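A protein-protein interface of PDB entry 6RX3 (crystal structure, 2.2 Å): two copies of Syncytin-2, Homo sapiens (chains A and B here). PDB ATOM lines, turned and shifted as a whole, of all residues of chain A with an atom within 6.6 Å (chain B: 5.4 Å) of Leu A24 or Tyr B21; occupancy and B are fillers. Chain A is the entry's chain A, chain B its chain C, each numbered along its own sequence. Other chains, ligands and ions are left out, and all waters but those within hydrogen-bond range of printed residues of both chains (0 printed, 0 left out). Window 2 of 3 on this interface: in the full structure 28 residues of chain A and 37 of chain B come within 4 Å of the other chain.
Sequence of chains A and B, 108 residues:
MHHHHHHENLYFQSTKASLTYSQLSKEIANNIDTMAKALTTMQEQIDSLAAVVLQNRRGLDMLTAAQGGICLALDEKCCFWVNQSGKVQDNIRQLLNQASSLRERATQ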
ATOM      1  N   THR A  20      -7.554  -0.163  -5.775  1.00  0.00           N
ATOM      2  CA  THR A  20      -6.381  -0.311  -6.642  1.00  0.00           C
ATOM      3  C   THR A  20      -6.775  -0.384  -8.125  1.00  0.00           C
ATOM      4  O   THR A  20      -7.935  -0.668  -8.441  1.00  0.00           O
ATOM      5  CB  THR A  20      -5.519  -1.532  -6.238  1.00  0.00           C
ATOM      6  OG1 THR A  20      -6.230  -2.747  -6.491  1.00  0.00           O
ATOM      7  CG2 THR A  20      -5.034  -1.473  -4.790  1.00  0.00           C
ATOM      8  N   TYR A  21      -5.789  -0.151  -9.024  1.00  0.00           N
ATOM      9  CA  TYR A  21      -5.924  -0.195 -10.478  1.00  0.00           C
ATOM     10  C   TYR A  21      -6.422  -1.565 -10.968  1.00  0.00           C
ATOM     11  O   TYR A  21      -7.455  -1.635 -11.641  1.00  0.00           O
ATOM     12  CB  TYR A  21      -4.582   0.168 -11.153  1.00  0.00           C
ATOM     13  CG  TYR A  21      -4.547  -0.081 -12.650  1.00  0.00           C
ATOM     14  CD1 TYR A  21      -5.032   0.867 -13.547  1.00  0.00           C
ATOM     15  CD2 TYR A  21      -4.024  -1.265 -13.170  1.00  0.00           C
ATOM     16  CE1 TYR A  21      -5.004   0.643 -14.924  1.00  0.00           C
ATOM     17  CE2 TYR A  21      -4.011  -1.510 -14.544  1.00  0.00           C
ATOM     18  CZ  TYR A  21      -4.493  -0.548 -15.418  1.00  0.00           C
ATOM     19  OH  TYR A  21      -4.471  -0.770 -16.776  1.00  0.00           O
ATOM     20  N   SER A  22      -5.665  -2.641 -10.653  1.00  0.00           N
ATOM     21  CA  SER A  22      -5.967  -4.005 -11.073  1.00  0.00           C
ATOM     22  C   SER A  22      -7.316  -4.498 -10.559  1.00  0.00           C
ATOM     23  O   SER A  22      -8.052  -5.107 -11.331  1.00  0.00           O
ATOM     24  CB  SER A  22      -4.831  -4.964 -10.710  1.00  0.00           C
ATOM     25  OG  SER A  22      -4.902  -5.473  -9.387  1.00  0.00           O
ATOM     26  N   GLN A  23      -7.657  -4.215  -9.284  1.00  0.00           N
ATOM     27  CA  GLN A  23      -8.943  -4.630  -8.722  1.00  0.00           C
ATOM     28  C   GLN A  23     -10.127  -3.878  -9.341  1.00  0.00           C
ATOM     29  O   GLN A  23     -11.213  -4.451  -9.437  1.00  0.00           O
ATOM     30  CB  GLN A  23      -8.965  -4.534  -7.188  1.00  0.00           C
ATOM     31  CG  GLN A  23      -8.371  -5.744  -6.478  1.00  0.00           C
ATOM     32  CD  GLN A  23      -9.160  -7.017  -6.711  1.00  0.00           C
ATOM     33  OE1 GLN A  23     -10.238  -7.232  -6.135  1.00  0.00           O
ATOM     34  NE2 GLN A  23      -8.642  -7.888  -7.575  1.00  0.00           N
ATOM     35  N   LEU A  24      -9.915  -2.604  -9.764  1.00  0.00           N
ATOM     36  CA  LEU A  24     -10.958  -1.788 -10.389  1.00  0.00           C
ATOM     37  C   LEU A  24     -11.237  -2.258 -11.816  1.00  0.00           C
ATOM     38  O   LEU A  24     -12.401  -2.497 -12.144  1.00  0.00           O
ATOM     39  CB  LEU A  24     -10.660  -0.272 -10.329  1.00  0.00           C
ATOM     40  CG  LEU A  24     -11.847   0.689 -10.573  1.00  0.00           C
ATOM     41  CD1 LEU A  24     -13.022   0.402  -9.640  1.00  0.00           C
ATOM     42  CD2 LEU A  24     -11.421   2.145 -10.418  1.00  0.00           C
ATOM     43  N   SER A  25     -10.178  -2.440 -12.640  1.00  0.00           N
ATOM     44  CA  SER A  25     -10.303  -2.925 -14.015  1.00  0.00           C
ATOM     45  C   SER A  25     -10.905  -4.340 -14.056  1.00  0.00           C
ATOM     46  O   SER A  25     -11.631  -4.653 -14.996  1.00  0.00           O
ATOM     47  CB  SER A  25      -8.967  -2.868 -14.746  1.00  0.00           C
ATOM     48  OG  SER A  25      -7.951  -3.509 -13.998  1.00  0.00           O
ATOM     49  N   LYS A  26     -10.656  -5.161 -13.010  1.00  0.00           N
ATOM     50  CA  LYS A  26     -11.230  -6.503 -12.883  1.00  0.00           C
ATOM     51  C   LYS A  26     -12.721  -6.428 -12.532  1.00  0.00           C
ATOM     52  O   LYS A  26     -13.493  -7.281 -12.979  1.00  0.00           O
ATOM     53  CB  LYS A  26     -10.445  -7.367 -11.884  1.00  0.00           C
ATOM     54  CG  LYS A  26      -9.181  -7.952 -12.507  1.00  0.00           C
ATOM     55  CD  LYS A  26      -8.223  -8.524 -11.477  1.00  0.00           C
ATOM     56  CE  LYS A  26      -6.935  -8.946 -12.141  1.00  0.00           C
ATOM     57  NZ  LYS A  26      -5.985  -9.561 -11.182  1.00  0.00           N
ATOM     58  N   GLU A  27     -13.128  -5.386 -11.772  1.00  0.00           N
ATOM     59  CA  GLU A  27     -14.521  -5.113 -11.404  1.00  0.00           C
ATOM     60  C   GLU A  27     -15.273  -4.551 -12.625  1.00  0.00           C
ATOM     61  O   GLU A  27     -16.417  -4.941 -12.875  1.00  0.00           O
ATOM     62  CB  GLU A  27     -14.585  -4.107 -10.238  1.00  0.00           C
ATOM     63  CG  GLU A  27     -14.452  -4.733  -8.858  1.00  0.00           C
ATOM     64  CD  GLU A  27     -15.701  -5.406  -8.326  1.00  0.00           C
ATOM     65  OE1 GLU A  27     -15.645  -6.630  -8.060  1.00  0.00           O
ATOM     66  OE2 GLU A  27     -16.734  -4.713  -8.173  1.00  0.00           O
ATOM     67  N   ILE A  28     -14.620  -3.629 -13.372  1.00  0.00           N
ATOM     68  CA  ILE A  28     -15.156  -2.988 -14.580  1.00  0.00           C
ATOM     69  C   ILE A  28     -15.415  -4.057 -15.643  1.00  0.00           C
ATOM     70  O   ILE A  28     -16.525  -4.102 -16.164  1.00  0.00           O
ATOM     71  CB  ILE A  28     -14.267  -1.808 -15.088  1.00  0.00           C
ATOM     72  CG1 ILE A  28     -14.244  -0.640 -14.080  1.00  0.00           C
ATOM     73  CG2 ILE A  28     -14.702  -1.306 -16.488  1.00  0.00           C
ATOM     74  CD1 ILE A  28     -12.982   0.232 -14.168  1.00  0.00           C
ATOM     75  N   ALA A  29     -14.427  -4.956 -15.898  1.00  0.00           N
ATOM     76  CA  ALA A  29     -14.531  -6.055 -16.864  1.00  0.00           C
ATOM     77  C   ALA A  29     -15.668  -7.051 -16.540  1.00  0.00           C
ATOM     78  O   ALA A  29     -16.298  -7.567 -17.466  1.00  0.00           O
ATOM     79  CB  ALA A  29     -13.205  -6.780 -16.985  1.00  0.00           C
ATOM     80  N   ALA B  17      -3.680   8.730  -4.658  1.00  0.00           N
ATOM     81  CA  ALA B  17      -4.001   7.694  -5.638  1.00  0.00           C
ATOM     82  C   ALA B  17      -5.254   6.922  -5.212  1.00  0.00           C
ATOM     83  O   ALA B  17      -6.079   6.581  -6.062  1.00  0.00           O
ATOM     84  CB  ALA B  17      -2.829   6.737  -5.790  1.00  0.00           C
ATOM     85  N   SER B  18      -5.386   6.642  -3.899  1.00  0.00           N
ATOM     86  CA  SER B  18      -6.511   5.929  -3.294  1.00  0.00           C
ATOM     87  C   SER B  18      -7.793   6.761  -3.421  1.00  0.00           C
ATOM     88  O   SER B  18      -8.854   6.199  -3.698  1.00  0.00           O
ATOM     89  CB  SER B  18      -6.212   5.619  -1.833  1.00  0.00           C
ATOM     90  OG  SER B  18      -7.164   4.728  -1.278  1.00  0.00           O
ATOM     91  N   LEU B  19      -7.677   8.100  -3.255  1.00  0.00           N
ATOM     92  CA  LEU B  19      -8.762   9.072  -3.384  1.00  0.00           C
ATOM     93  C   LEU B  19      -9.254   9.148  -4.841  1.00  0.00           C
ATOM     94  O   LEU B  19     -10.465   9.188  -5.063  1.00  0.00           O
ATOM     95  CB  LEU B  19      -8.309  10.454  -2.852  1.00  0.00           C
ATOM     96  CG  LEU B  19      -9.069  11.725  -3.301  1.00  0.00           C
ATOM     97  CD1 LEU B  19     -10.496  11.783  -2.725  1.00  0.00           C
ATOM     98  CD2 LEU B  19      -8.299  12.980  -2.916  1.00  0.00           C
ATOM     99  N   THR B  20      -8.327   9.161  -5.822  1.00  0.00           N
ATOM    100  CA  THR B  20      -8.701   9.190  -7.244  1.00  0.00           C
ATOM    101  C   THR B  20      -9.476   7.921  -7.624  1.00  0.00           C
ATOM    102  O   THR B  20     -10.490   8.032  -8.312  1.00  0.00           O
ATOM    103  CB  THR B  20      -7.511   9.453  -8.182  1.00  0.00           C
ATOM    104  OG1 THR B  20      -6.490   8.488  -7.945  1.00  0.00           O
ATOM    105  CG2 THR B  20      -6.957  10.870  -8.064  1.00  0.00           C
ATOM    106  N   TYR B  21      -9.034   6.736  -7.131  1.00  0.00           N
ATOM    107  CA  TYR B  21      -9.723   5.478  -7.410  1.00  0.00           C
ATOM    108  C   TYR B  21     -11.069   5.383  -6.693  1.00  0.00           C
ATOM    109  O   TYR B  21     -12.004   4.809  -7.247  1.00  0.00           O
ATOM    110  CB  TYR B  21      -8.834   4.252  -7.152  1.00  0.00           C
ATOM    111  CG  TYR B  21      -7.786   4.054  -8.231  1.00  0.00           C
ATOM    112  CD1 TYR B  21      -8.137   4.042  -9.582  1.00  0.00           C
ATOM    113  CD2 TYR B  21      -6.444   3.872  -7.904  1.00  0.00           C
ATOM    114  CE1 TYR B  21      -7.174   3.888 -10.580  1.00  0.00           C
ATOM    115  CE2 TYR B  21      -5.473   3.716  -8.895  1.00  0.00           C
ATOM    116  CZ  TYR B  21      -5.844   3.721 -10.232  1.00  0.00           C
ATOM    117  OH  TYR B  21      -4.898   3.564 -11.218  1.00  0.00           O
ATOM    118  N   SER B  22     -11.187   5.993  -5.503  1.00  0.00           N
ATOM    119  CA  SER B  22     -12.439   6.041  -4.741  1.00  0.00           C
ATOM    120  C   SER B  22     -13.460   6.906  -5.503  1.00  0.00           C
ATOM    121  O   SER B  22     -14.618   6.516  -5.630  1.00  0.00           O
ATOM    122  CB  SER B  22     -12.192   6.590  -3.336  1.00  0.00           C
ATOM    123  OG  SER B  22     -13.362   7.097  -2.715  1.00  0.00           O
ATOM    124  N   GLN B  23     -13.012   8.052  -6.043  1.00  0.00           N
ATOM    125  CA  GLN B  23     -13.854   8.969  -6.808  1.00  0.00           C
ATOM    126  C   GLN B  23     -14.227   8.396  -8.179  1.00  0.00           C
ATOM    127  O   GLN B  23     -15.353   8.600  -8.635  1.00  0.00           O
ATOM    128  CB  GLN B  23     -13.194  10.356  -6.940  1.00  0.00           C
ATOM    129  CG  GLN B  23     -13.182  11.178  -5.643  1.00  0.00           C
ATOM    130  CD  GLN B  23     -14.568  11.455  -5.088  1.00  0.00           C
ATOM    131  OE1 GLN B  23     -15.343  12.255  -5.634  1.00  0.00           O
ATOM    132  NE2 GLN B  23     -14.909  10.797  -3.987  1.00  0.00           N
ATOM    133  N   LEU B  24     -13.292   7.665  -8.814  1.00  0.00           N
ATOM    134  CA  LEU B  24     -13.497   7.023 -10.111  1.00  0.00           C
ATOM    135  C   LEU B  24     -14.541   5.903 -10.015  1.00  0.00           C
ATOM    136  O   LEU B  24     -15.402   5.813 -10.895  1.00  0.00           O
ATOM    137  CB  LEU B  24     -12.170   6.496 -10.695  1.00  0.00           C
ATOM    138  CG  LEU B  24     -12.217   5.929 -12.124  1.00  0.00           C
ATOM    139  CD1 LEU B  24     -12.614   6.999 -13.157  1.00  0.00           C
ATOM    140  CD2 LEU B  24     -10.903   5.308 -12.495  1.00  0.00           C
ATOM    141  N   SER B  25     -14.478   5.083  -8.936  1.00  0.00           N
ATOM    142  CA  SER B  25     -15.409   3.981  -8.684  1.00  0.00           C
ATOM    143  C   SER B  25     -16.816   4.465  -8.332  1.00  0.00           C
ATOM    144  O   SER B  25     -17.772   3.742  -8.616  1.00  0.00           O
ATOM    145  CB  SER B  25     -14.865   3.005  -7.644  1.00  0.00           C
ATOM    146  OG  SER B  25     -14.583   3.633  -6.409  1.00  0.00           O
ATOM    147  N   LYS B  26     -16.950   5.695  -7.770  1.00  0.00           N
ATOM    148  CA  LYS B  26     -18.245   6.321  -7.473  1.00  0.00           C
ATOM    149  C   LYS B  26     -18.946   6.677  -8.792  1.00  0.00           C
ATOM    150  O   LYS B  26     -20.161   6.509  -8.908  1.00  0.00           O
ATOM    151  CB  LYS B  26     -18.075   7.585  -6.607  1.00  0.00           C
ATOM    152  CG  LYS B  26     -18.038   7.298  -5.117  1.00  0.00           C
ATOM    153  CD  LYS B  26     -17.518   8.480  -4.307  1.00  0.00           C
ATOM    154  CE  LYS B  26     -17.195   8.039  -2.896  1.00  0.00           C
ATOM    155  NZ  LYS B  26     -16.698   9.151  -2.044  1.00  0.00           N
ATOM    156  N   ILE B  28     -18.331   5.178 -11.785  1.00  0.00           N
ATOM    157  CA  ILE B  28     -18.613   3.887 -12.419  1.00  0.00           C
ATOM    158  C   ILE B  28     -19.938   3.352 -11.875  1.00  0.00           C
ATOM    159  O   ILE B  28     -20.777   2.914 -12.663  1.00  0.00           O
ATOM    160  CB  ILE B  28     -17.434   2.885 -12.236  1.00  0.00           C
ATOM    161  CG1 ILE B  28     -16.188   3.356 -13.037  1.00  0.00           C
ATOM    162  CG2 ILE B  28     -17.830   1.444 -12.636  1.00  0.00           C
ATOM    163  CD1 ILE B  28     -14.847   2.920 -12.455  1.00  0.00           C
ATOM    164  N   LEU B 102     -19.475  -1.323  -5.169  1.00  0.00           N
ATOM    165  CA  LEU B 102     -18.422  -0.354  -5.517  1.00  0.00           C
ATOM    166  C   LEU B 102     -18.587   0.932  -4.705  1.00  0.00           C
ATOM    167  O   LEU B 102     -17.600   1.472  -4.215  1.00  0.00           O
ATOM    168  CB  LEU B 102     -18.444   0.002  -7.015  1.00  0.00           C
ATOM    169  CG  LEU B 102     -17.396  -0.607  -7.948  1.00  0.00           C
ATOM    170  CD1 LEU B 102     -17.333   0.177  -9.230  1.00  0.00           C
ATOM    171  CD2 LEU B 102     -15.999  -0.633  -7.327  1.00  0.00           C
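Hydrophobic or aromatic side chains of chain A that line the printed part of chain B: Tyr A21, Leu A24 and Ile A28. Along chain A the printed residues that touch a printed residue of chain B span positions 21 to 28. Of the 12 printed residues of chain B, 5 touch a printed residue of chain A. Among the printed residues, 6 pairs touch across the chains. Among the printed residues, no Asp or Glu carboxylate lies within 4 Å of a Lys or Arg side-chain nitrogen of the other chain.
The backbone carbonyl oxygen (O) of Tyr B21 is in hydrogen-bond range of the side-chain hydroxyl (OG) of Ser B25. OG of Ser B25 lies within hydrogen-bond range of O of Ser B22, at 3.0 Å. O of Tyr A21 lies within hydrogen-bond range of OG of Ser A25 (3.1 Å).
Tyr B21 touches its own counterpart, Tyr A21. Leu A24 touches its own counterpart, Leu B24. Leu A24 touches Ser B25, but with the chains exchanged Ser A25 does not touch Leu B24 (7.8 Å). Ile B28 touches its own counterpart, Ile A28. Of the 6 pairs that touch across the chains among the printed residues, 3 have their exchanged pair printed and touching as well.
CB of Tyr A21 touches OH of Tyr B21, 3.4 Å away. Leu A24 touches Tyr B21 (CD2 to CD1, 3.9 Å). Leu B24 touches Leu A24. Leu A24 touches Ser B25. CD1 of Leu A24 touches CD2 of Leu B102, 3.9 Å away. Ile A28 touches Ile B28.
Thr A20 touches none of the printed residues of chain B. Of the printed residues of chain B, Ile A28 touches Ile B28 (3.7 Å). Tyr B21 touches just these residues of chain A: Tyr A21 and Leu A24. Ser B22 touches none of the printed residues of chain A. Printed residues of chain A within 4 Å of Ile B28: Ile A28 (3.7 Å). The nearest residue of chain A that does not touch Tyr B21 is Thr A20 (4.3 Å).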
